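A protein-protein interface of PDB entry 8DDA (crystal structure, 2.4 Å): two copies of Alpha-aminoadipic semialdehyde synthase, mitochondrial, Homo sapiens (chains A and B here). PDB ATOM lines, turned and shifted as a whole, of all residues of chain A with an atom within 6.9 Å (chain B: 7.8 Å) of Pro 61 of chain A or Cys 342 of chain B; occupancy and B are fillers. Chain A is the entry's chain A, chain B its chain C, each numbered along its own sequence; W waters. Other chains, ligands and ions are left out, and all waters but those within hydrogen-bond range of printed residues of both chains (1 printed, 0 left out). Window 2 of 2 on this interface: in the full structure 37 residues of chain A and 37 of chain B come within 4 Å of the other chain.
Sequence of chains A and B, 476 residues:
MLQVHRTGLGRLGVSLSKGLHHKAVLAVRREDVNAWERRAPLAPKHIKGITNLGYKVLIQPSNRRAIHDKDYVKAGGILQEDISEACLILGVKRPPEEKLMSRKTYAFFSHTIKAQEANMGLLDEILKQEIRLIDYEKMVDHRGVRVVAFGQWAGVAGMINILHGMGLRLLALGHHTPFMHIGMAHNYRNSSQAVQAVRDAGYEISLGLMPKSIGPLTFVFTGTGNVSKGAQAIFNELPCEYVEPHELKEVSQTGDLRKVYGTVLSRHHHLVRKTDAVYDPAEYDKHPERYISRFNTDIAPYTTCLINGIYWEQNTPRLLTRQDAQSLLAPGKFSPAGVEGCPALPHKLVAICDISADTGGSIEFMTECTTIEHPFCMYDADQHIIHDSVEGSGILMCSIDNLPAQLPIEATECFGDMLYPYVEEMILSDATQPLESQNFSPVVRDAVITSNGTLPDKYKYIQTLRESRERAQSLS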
ATOM      1  N   VAL A  28      12.340 -17.225  -4.270  1.00  0.00           N
ATOM      2  CA  VAL A  28      13.582 -16.454  -3.971  1.00  0.00           C
ATOM      3  C   VAL A  28      13.415 -15.859  -2.572  1.00  0.00           C
ATOM      4  O   VAL A  28      12.514 -15.016  -2.408  1.00  0.00           O
ATOM      5  CB  VAL A  28      13.839 -15.358  -5.027  1.00  0.00           C
ATOM      6  CG1 VAL A  28      15.118 -14.569  -4.745  1.00  0.00           C
ATOM      7  CG2 VAL A  28      13.861 -15.944  -6.436  1.00  0.00           C
ATOM      8  N   ARG A  29      14.249 -16.285  -1.617  1.00  0.00           N
ATOM      9  CA  ARG A  29      14.202 -15.842  -0.197  1.00  0.00           C
ATOM     10  C   ARG A  29      14.857 -14.455  -0.052  1.00  0.00           C
ATOM     11  O   ARG A  29      15.746 -14.093  -0.876  1.00  0.00           O
ATOM     12  CB  ARG A  29      14.967 -16.844   0.676  1.00  0.00           C
ATOM     13  CG  ARG A  29      14.285 -17.326   1.943  1.00  0.00           C
ATOM     14  CD  ARG A  29      15.181 -18.386   2.588  1.00  0.00           C
ATOM     15  NE  ARG A  29      16.435 -17.767   3.001  1.00  0.00           N
ATOM     16  CZ  ARG A  29      16.700 -17.295   4.217  1.00  0.00           C
ATOM     17  NH1 ARG A  29      15.825 -17.422   5.203  1.00  0.00           N
ATOM     18  NH2 ARG A  29      17.850 -16.684   4.445  1.00  0.00           N
ATOM     19  N   ARG A  30      14.428 -13.710   0.970  1.00  0.00           N
ATOM     20  CA  ARG A  30      15.077 -12.461   1.439  1.00  0.00           C
ATOM     21  C   ARG A  30      16.412 -12.825   2.096  1.00  0.00           C
ATOM     22  O   ARG A  30      16.452 -13.829   2.801  1.00  0.00           O
ATOM     23  CB  ARG A  30      14.154 -11.728   2.417  1.00  0.00           C
ATOM     24  CG  ARG A  30      14.799 -10.509   3.060  1.00  0.00           C
ATOM     25  CD  ARG A  30      13.815  -9.708   3.889  1.00  0.00           C
ATOM     26  NE  ARG A  30      13.150 -10.557   4.874  1.00  0.00           N
ATOM     27  CZ  ARG A  30      11.887 -10.979   4.814  1.00  0.00           C
ATOM     28  NH1 ARG A  30      11.084 -10.635   3.812  1.00  0.00           N
ATOM     29  NH2 ARG A  30      11.428 -11.744   5.788  1.00  0.00           N
ATOM     30  N   ILE A  59       8.395 -14.352  -4.737  1.00  0.00           N
ATOM     31  CA  ILE A  59       9.519 -13.465  -4.330  1.00  0.00           C
ATOM     32  C   ILE A  59       9.171 -12.885  -2.961  1.00  0.00           C
ATOM     33  O   ILE A  59       8.135 -12.220  -2.838  1.00  0.00           O
ATOM     34  CB  ILE A  59       9.782 -12.410  -5.414  1.00  0.00           C
ATOM     35  CG1 ILE A  59      10.346 -13.086  -6.670  1.00  0.00           C
ATOM     36  CG2 ILE A  59      10.694 -11.297  -4.913  1.00  0.00           C
ATOM     37  CD1 ILE A  59       9.655 -12.670  -7.948  1.00  0.00           C
ATOM     38  N   GLN A  60       9.996 -13.196  -1.965  1.00  0.00           N
ATOM     39  CA  GLN A  60       9.869 -12.708  -0.571  1.00  0.00           C
ATOM     40  C   GLN A  60      10.290 -11.233  -0.557  1.00  0.00           C
ATOM     41  O   GLN A  60      11.377 -10.898  -1.030  1.00  0.00           O
ATOM     42  CB  GLN A  60      10.713 -13.620   0.330  1.00  0.00           C
ATOM     43  CG  GLN A  60      10.204 -13.736   1.758  1.00  0.00           C
ATOM     44  CD  GLN A  60      10.896 -14.863   2.494  1.00  0.00           C
ATOM     45  OE1 GLN A  60      12.115 -15.012   2.451  1.00  0.00           O
ATOM     46  NE2 GLN A  60      10.111 -15.682   3.179  1.00  0.00           N
ATOM     47  N   PRO A  61       9.446 -10.305  -0.053  1.00  0.00           N
ATOM     48  CA  PRO A  61       9.722  -8.867  -0.165  1.00  0.00           C
ATOM     49  C   PRO A  61      10.983  -8.447   0.605  1.00  0.00           C
ATOM     50  O   PRO A  61      11.209  -8.967   1.678  1.00  0.00           O
ATOM     51  CB  PRO A  61       8.507  -8.162   0.469  1.00  0.00           C
ATOM     52  CG  PRO A  61       7.462  -9.256   0.693  1.00  0.00           C
ATOM     53  CD  PRO A  61       8.180 -10.595   0.644  1.00  0.00           C
ATOM     54  N   SER A  62      11.766  -7.517   0.053  1.00  0.00           N
ATOM     55  CA  SER A  62      13.092  -7.134   0.591  1.00  0.00           C
ATOM     56  C   SER A  62      13.451  -5.692   0.210  1.00  0.00           C
ATOM     57  O   SER A  62      13.714  -5.457  -0.977  1.00  0.00           O
ATOM     58  CB  SER A  62      14.155  -8.099   0.114  1.00  0.00           C
ATOM     59  OG  SER A  62      15.419  -7.761   0.633  1.00  0.00           O
ATOM     60  N   ASN A  63      13.515  -4.788   1.190  1.00  0.00           N
ATOM     61  CA  ASN A  63      14.137  -3.449   1.031  1.00  0.00           C
ATOM     62  C   ASN A  63      15.652  -3.576   0.877  1.00  0.00           C
ATOM     63  O   ASN A  63      16.272  -2.581   0.485  1.00  0.00           O
ATOM     64  CB  ASN A  63      13.815  -2.516   2.200  1.00  0.00           C
ATOM     65  CG  ASN A  63      12.361  -2.097   2.257  1.00  0.00           C
ATOM     66  OD1 ASN A  63      11.557  -2.488   1.413  1.00  0.00           O
ATOM     67  ND2 ASN A  63      12.012  -1.329   3.281  1.00  0.00           N
ATOM     68  N   ARG A  64      16.244  -4.730   1.196  1.00  0.00           N
ATOM     69  CA  ARG A  64      17.721  -4.914   1.201  1.00  0.00           C
ATOM     70  C   ARG A  64      18.248  -5.078  -0.235  1.00  0.00           C
ATOM     71  O   ARG A  64      19.372  -4.615  -0.504  1.00  0.00           O
ATOM     72  CB  ARG A  64      18.108  -6.125   2.057  1.00  0.00           C
ATOM     73  CG  ARG A  64      19.605  -6.221   2.328  1.00  0.00           C
ATOM     74  CD  ARG A  64      20.002  -7.181   3.424  1.00  0.00           C
ATOM     75  NE  ARG A  64      19.244  -6.744   4.584  1.00  0.00           N
ATOM     76  CZ  ARG A  64      19.301  -7.253   5.789  1.00  0.00           C
ATOM     77  NH1 ARG A  64      20.136  -8.238   6.078  1.00  0.00           N
ATOM     78  NH2 ARG A  64      18.515  -6.765   6.728  1.00  0.00           N
ATOM     79  N   ARG A  65      17.472  -5.721  -1.115  1.00  0.00           N
ATOM     80  CA  ARG A  65      17.908  -6.090  -2.491  1.00  0.00           C
ATOM     81  C   ARG A  65      18.118  -4.816  -3.316  1.00  0.00           C
ATOM     82  O   ARG A  65      17.295  -3.905  -3.210  1.00  0.00           O
ATOM     83  CB  ARG A  65      16.901  -7.032  -3.159  1.00  0.00           C
ATOM     84  CG  ARG A  65      17.506  -7.958  -4.207  1.00  0.00           C
ATOM     85  CD  ARG A  65      16.453  -8.646  -5.060  1.00  0.00           C
ATOM     86  NE  ARG A  65      15.366  -9.226  -4.276  1.00  0.00           N
ATOM     87  CZ  ARG A  65      14.154  -8.678  -4.090  1.00  0.00           C
ATOM     88  NH1 ARG A  65      13.244  -9.294  -3.344  1.00  0.00           N
ATOM     89  NH2 ARG A  65      13.858  -7.510  -4.629  1.00  0.00           N
ATOM     90  N   ASP A  69      11.599  -4.743  -5.732  1.00  0.00           N
ATOM     91  CA  ASP A  69      10.562  -5.811  -5.786  1.00  0.00           C
ATOM     92  C   ASP A  69       9.683  -5.648  -7.040  1.00  0.00           C
ATOM     93  O   ASP A  69       9.382  -6.672  -7.688  1.00  0.00           O
ATOM     94  CB  ASP A  69       9.707  -5.817  -4.504  1.00  0.00           C
ATOM     95  CG  ASP A  69      10.407  -6.347  -3.259  1.00  0.00           C
ATOM     96  OD1 ASP A  69      11.295  -7.234  -3.388  1.00  0.00           O
ATOM     97  OD2 ASP A  69      10.036  -5.878  -2.169  1.00  0.00           O
ATOM     98  N   LEU A  79       4.708 -11.296  -5.206  1.00  0.00           N
ATOM     99  CA  LEU A  79       5.361 -10.769  -3.975  1.00  0.00           C
ATOM    100  C   LEU A  79       4.565 -11.258  -2.763  1.00  0.00           C
ATOM    101  O   LEU A  79       3.370 -10.932  -2.685  1.00  0.00           O
ATOM    102  CB  LEU A  79       5.389  -9.237  -4.057  1.00  0.00           C
ATOM    103  CG  LEU A  79       6.403  -8.539  -3.156  1.00  0.00           C
ATOM    104  CD1 LEU A  79       7.824  -8.783  -3.647  1.00  0.00           C
ATOM    105  CD2 LEU A  79       6.125  -7.040  -3.084  1.00  0.00           C
ATOM    106  N   GLN A  80       5.188 -12.020  -1.863  1.00  0.00           N
ATOM    107  CA  GLN A  80       4.469 -12.746  -0.778  1.00  0.00           C
ATOM    108  C   GLN A  80       5.469 -13.198   0.289  1.00  0.00           C
ATOM    109  O   GLN A  80       6.507 -13.775  -0.080  1.00  0.00           O
ATOM    110  CB  GLN A  80       3.692 -13.898  -1.422  1.00  0.00           C
ATOM    111  CG  GLN A  80       3.282 -15.020  -0.475  1.00  0.00           C
ATOM    112  CD  GLN A  80       2.477 -16.088  -1.182  1.00  0.00           C
ATOM    113  OE1 GLN A  80       1.706 -15.810  -2.099  1.00  0.00           O
ATOM    114  NE2 GLN A  80       2.647 -17.329  -0.761  1.00  0.00           N
ATOM    115  N   GLU A  81       5.155 -12.937   1.563  1.00  0.00           N
ATOM    116  CA  GLU A  81       6.026 -13.260   2.727  1.00  0.00           C
ATOM    117  C   GLU A  81       6.049 -14.774   2.949  1.00  0.00           C
ATOM    118  O   GLU A  81       7.148 -15.300   3.193  1.00  0.00           O
ATOM    119  CB  GLU A  81       5.565 -12.541   4.001  1.00  0.00           C
ATOM    120  CG  GLU A  81       6.507 -12.747   5.174  1.00  0.00           C
ATOM    121  CD  GLU A  81       7.944 -12.311   4.911  1.00  0.00           C
ATOM    122  OE1 GLU A  81       8.133 -11.265   4.250  1.00  0.00           O
ATOM    123  OE2 GLU A  81       8.887 -13.035   5.325  1.00  0.00           O
ATOM    124  N   ASP A  82       4.886 -15.433   2.878  1.00  0.00           N
ATOM    125  CA  ASP A  82       4.731 -16.889   3.170  1.00  0.00           C
ATOM    126  C   ASP A  82       5.198 -17.696   1.953  1.00  0.00           C
ATOM    127  O   ASP A  82       4.511 -17.635   0.927  1.00  0.00           O
ATOM    128  CB  ASP A  82       3.296 -17.250   3.580  1.00  0.00           C
ATOM    129  CG  ASP A  82       3.085 -18.709   3.979  1.00  0.00           C
ATOM    130  OD1 ASP A  82       4.093 -19.430   4.089  1.00  0.00           O
ATOM    131  OD2 ASP A  82       1.921 -19.130   4.069  1.00  0.00           O
ATOM    132  N   ILE A  83       6.288 -18.458   2.106  1.00  0.00           N
ATOM    133  CA  ILE A  83       6.933 -19.247   1.015  1.00  0.00           C
ATOM    134  C   ILE A  83       6.866 -20.737   1.391  1.00  0.00           C
ATOM    135  O   ILE A  83       7.746 -21.539   0.962  1.00  0.00           O
ATOM    136  CB  ILE A  83       8.372 -18.745   0.747  1.00  0.00           C
ATOM    137  CG1 ILE A  83       9.274 -18.803   1.979  1.00  0.00           C
ATOM    138  CG2 ILE A  83       8.356 -17.343   0.169  1.00  0.00           C
ATOM    139  CD1 ILE A  83      10.738 -18.752   1.629  1.00  0.00           C
ATOM    140  N   GLY B 174      18.517  -1.861   7.132  1.00  0.00           N
ATOM    141  CA  GLY B 174      17.972  -2.879   6.209  1.00  0.00           C
ATOM    142  C   GLY B 174      17.377  -2.309   4.925  1.00  0.00           C
ATOM    143  O   GLY B 174      16.562  -3.005   4.303  1.00  0.00           O
ATOM    144  N   HIS B 175      17.763  -1.112   4.485  1.00  0.00           N
ATOM    145  CA  HIS B 175      17.131  -0.423   3.324  1.00  0.00           C
ATOM    146  C   HIS B 175      18.192  -0.003   2.309  1.00  0.00           C
ATOM    147  O   HIS B 175      18.912   0.987   2.562  1.00  0.00           O
ATOM    148  CB  HIS B 175      16.307   0.785   3.791  1.00  0.00           C
ATOM    149  CG  HIS B 175      15.477   0.525   4.997  1.00  0.00           C
ATOM    150  ND1 HIS B 175      14.252  -0.093   4.922  1.00  0.00           N
ATOM    151  CD2 HIS B 175      15.693   0.806   6.300  1.00  0.00           C
ATOM    152  CE1 HIS B 175      13.743  -0.197   6.139  1.00  0.00           C
ATOM    153  NE2 HIS B 175      14.616   0.342   7.004  1.00  0.00           N
ATOM    154  N   PRO B 211      12.368   2.488  -1.118  1.00  0.00           N
ATOM    155  CA  PRO B 211      11.433   1.582  -0.447  1.00  0.00           C
ATOM    156  C   PRO B 211      10.287   2.357   0.218  1.00  0.00           C
ATOM    157  O   PRO B 211      10.569   3.355   0.848  1.00  0.00           O
ATOM    158  CB  PRO B 211      12.308   0.894   0.608  1.00  0.00           C
ATOM    159  CG  PRO B 211      13.383   1.895   0.904  1.00  0.00           C
ATOM    160  CD  PRO B 211      13.657   2.579  -0.420  1.00  0.00           C
ATOM    161  N   LYS B 212       9.038   1.900   0.042  1.00  0.00           N
ATOM    162  CA  LYS B 212       7.811   2.591   0.514  1.00  0.00           C
ATOM    163  C   LYS B 212       7.761   2.648   2.041  1.00  0.00           C
ATOM    164  O   LYS B 212       7.312   3.703   2.557  1.00  0.00           O
ATOM    165  CB  LYS B 212       6.559   1.867   0.027  1.00  0.00           C
ATOM    166  CG  LYS B 212       6.312   1.982  -1.468  1.00  0.00           C
ATOM    167  CD  LYS B 212       4.992   1.313  -1.880  1.00  0.00           C
ATOM    168  CE  LYS B 212       4.778   1.264  -3.381  1.00  0.00           C
ATOM    169  NZ  LYS B 212       4.744   2.619  -3.978  1.00  0.00           N
ATOM    170  N   SER B 213       8.153   1.564   2.724  1.00  0.00           N
ATOM    171  CA  SER B 213       7.916   1.350   4.178  1.00  0.00           C
ATOM    172  C   SER B 213       8.560   2.458   5.026  1.00  0.00           C
ATOM    173  O   SER B 213       8.075   2.703   6.128  1.00  0.00           O
ATOM    174  CB  SER B 213       8.384  -0.023   4.633  1.00  0.00           C
ATOM    175  OG  SER B 213       9.809  -0.107   4.647  1.00  0.00           O
ATOM    176  N   ILE B 214       9.620   3.085   4.524  1.00  0.00           N
ATOM    177  CA  ILE B 214      10.430   4.147   5.183  1.00  0.00           C
ATOM    178  C   ILE B 214       9.692   5.491   5.221  1.00  0.00           C
ATOM    179  O   ILE B 214      10.065   6.316   6.070  1.00  0.00           O
ATOM    180  CB  ILE B 214      11.777   4.230   4.444  1.00  0.00           C
ATOM    181  CG1 ILE B 214      12.755   3.215   5.034  1.00  0.00           C
ATOM    182  CG2 ILE B 214      12.368   5.630   4.400  1.00  0.00           C
ATOM    183  CD1 ILE B 214      14.171   3.381   4.491  1.00  0.00           C
ATOM    184  N   GLY B 341      11.093  -7.600   6.792  1.00  0.00           N
ATOM    185  CA  GLY B 341      11.569  -7.485   5.397  1.00  0.00           C
ATOM    186  C   GLY B 341      11.312  -6.103   4.813  1.00  0.00           C
ATOM    187  O   GLY B 341      12.076  -5.670   3.895  1.00  0.00           O
ATOM    188  N   CYS B 342      10.294  -5.417   5.343  1.00  0.00           N
ATOM    189  CA  CYS B 342       9.904  -4.037   4.945  1.00  0.00           C
ATOM    190  C   CYS B 342       9.451  -3.257   6.178  1.00  0.00           C
ATOM    191  O   CYS B 342       8.296  -2.853   6.286  1.00  0.00           O
ATOM    192  CB  CYS B 342       8.827  -4.081   3.865  1.00  0.00           C
ATOM    193  SG  CYS B 342       9.292  -5.145   2.474  1.00  0.00           S
ATOM    194  N   PRO B 343      10.351  -3.048   7.159  1.00  0.00           N
ATOM    195  CA  PRO B 343       9.988  -2.327   8.375  1.00  0.00           C
ATOM    196  C   PRO B 343       9.894  -0.809   8.149  1.00  0.00           C
ATOM    197  O   PRO B 343      10.509  -0.294   7.201  1.00  0.00           O
ATOM    198  CB  PRO B 343      11.125  -2.679   9.350  1.00  0.00           C
ATOM    199  CG  PRO B 343      12.321  -2.993   8.474  1.00  0.00           C
ATOM    200  CD  PRO B 343      11.746  -3.522   7.172  1.00  0.00           C
ATOM    201  N   ALA B 344       9.118  -0.137   9.001  1.00  0.00           N
ATOM    202  CA  ALA B 344       9.149   1.326   9.189  1.00  0.00           C
ATOM    203  C   ALA B 344      10.474   1.668   9.871  1.00  0.00           C
ATOM    204  O   ALA B 344      11.063   0.727  10.427  1.00  0.00           O
ATOM    205  CB  ALA B 344       7.951   1.777  10.001  1.00  0.00           C
ATOM    206  N   LEU B 345      10.915   2.931   9.817  1.00  0.00           N
ATOM    207  CA  LEU B 345      12.035   3.463  10.639  1.00  0.00           C
ATOM    208  C   LEU B 345      11.688   3.285  12.113  1.00  0.00           C
ATOM    209  O   LEU B 345      10.521   3.397  12.477  1.00  0.00           O
ATOM    210  CB  LEU B 345      12.285   4.945  10.321  1.00  0.00           C
ATOM    211  CG  LEU B 345      12.861   5.263   8.938  1.00  0.00           C
ATOM    212  CD1 LEU B 345      12.834   6.765   8.679  1.00  0.00           C
ATOM    213  CD2 LEU B 345      14.280   4.714   8.782  1.00  0.00           C
HETATM  214  O   HOH W   1       9.187  -0.943   1.382  1.00  0.00           O
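The side-chain amide nitrogen (ND2) of Asn 63 of chain A lies within hydrogen-bond range of a ring nitrogen (ND1) of His 175 of chain B (3.0 Å). The side-chain hydroxyl (OG) of Ser 213 of chain B lies within hydrogen-bond range of the side-chain amide nitrogen (ND2) of Asn 63 of chain A. The backbone NH (N) of Asn 63 of chain A lies within hydrogen-bond range of the backbone carbonyl oxygen (O) of Gly 341 of chain B (3.2 Å). The side-chain amide oxygen (OD1) of Asn 63 of chain A lies within hydrogen-bond range of the side-chain sulfur (SG) of Cys 342 of chain B.
The backbone NH of Arg 30 of chain A is in hydrogen-bond range of the side-chain amide oxygen of Gln 60 of chain A, at 3.0 Å. NH2 of Arg 30 of chain A is in salt-bridge range of OE2 of Glu 81 of chain A (2.9 Å). The side-chain hydroxyl (OG) of Ser 62 of chain A lies close to the backbone NH (N) of Arg 64 of chain A (3.2 Å). OG of Ser 62 of chain A is in hydrogen-bond range of N of Arg 65 of chain A, 3.4 Å away. The side-chain carboxylate (OD2) of Asp 69 of chain A lies within hydrogen-bond range of the backbone NH (N) of Ser 62 of chain A (3.3 Å). The side-chain hydroxyl (OG) of Ser 213 of chain B sits at hydrogen-bond distance from the backbone carbonyl oxygen (O) of Pro 343 of chain B (2.7 Å).
NE of Arg 30 of chain A touches CA of Gly 341 of chain B, 3.5 Å away. Cys 342 of chain B touches Pro 61 of chain A. Ser 62 of chain A touches Gly 341 of chain B. O of Gly 174 of chain B touches CB of Asn 63 of chain A, 3.5 Å away. Pro 211 of chain B touches Asn 63 of chain A. Gly 174 of chain B touches Arg 64 of chain A (O to N, 3.6 Å).
Of the printed residues of chain B, Pro 61 of chain A touches Cys 342 (3.7 Å). Printed residues of chain A within 4 Å of Cys 342 of chain B: Pro 61 and Asn 63. Of the printed residues of chain B, Arg 30 of chain A touches Gly 341 (3.5 Å). Of the printed residues of chain A, Ser 213 of chain B touches Asn 63 (2.9 Å). Of the printed residues of chain A, His 175 of chain B touches Asn 63 (3.0 Å). Of the printed residues of chain A, Pro 211 of chain B touches Asn 63 (3.4 Å). Printed residues of chain A within 4 Å of Gly 174 of chain B: Asn 63 and Arg 64. Gln 60 of chain A touches none of the printed residues of chain B. Ile 83 of chain A touches none of the printed residues of chain B. The nearest printed residue of chain B that does not touch Pro 61 of chain A is Gly 341 of chain B (4.02 Å). The nearest residue of chain A that does not touch Cys 342 of chain B is Ser 62 of chain A (4.2 Å).
Along chain A the printed residues that touch a printed residue of chain B span positions 30 to 64. Of the 11 printed residues of chain B, 6 touch a printed residue of chain A. Hydrophobic or aromatic side chains of chain B that line the printed part of chain A: His 175 and Pro 211. Among the printed residues, 10 pairs touch across the chains. Among the printed residues, no Asp or Glu carboxylate lies within 4 Å of a Lys or Arg side-chain nitrogen of the other chain.
No position is printed for both chains. Of the 10 pairs that touch across the chains among the printed residues, none has its exchanged pair printed and touching as well.
Water W1 lies within hydrogen-bond range of the side-chain amide oxygen (OD1) of Asn 63 of chain A (2.8 Å), the backbone NH (N) of Ser 213 of chain B (3.0 Å) and the backbone NH (N) of Lys 212 of chain B (3.1 Å).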
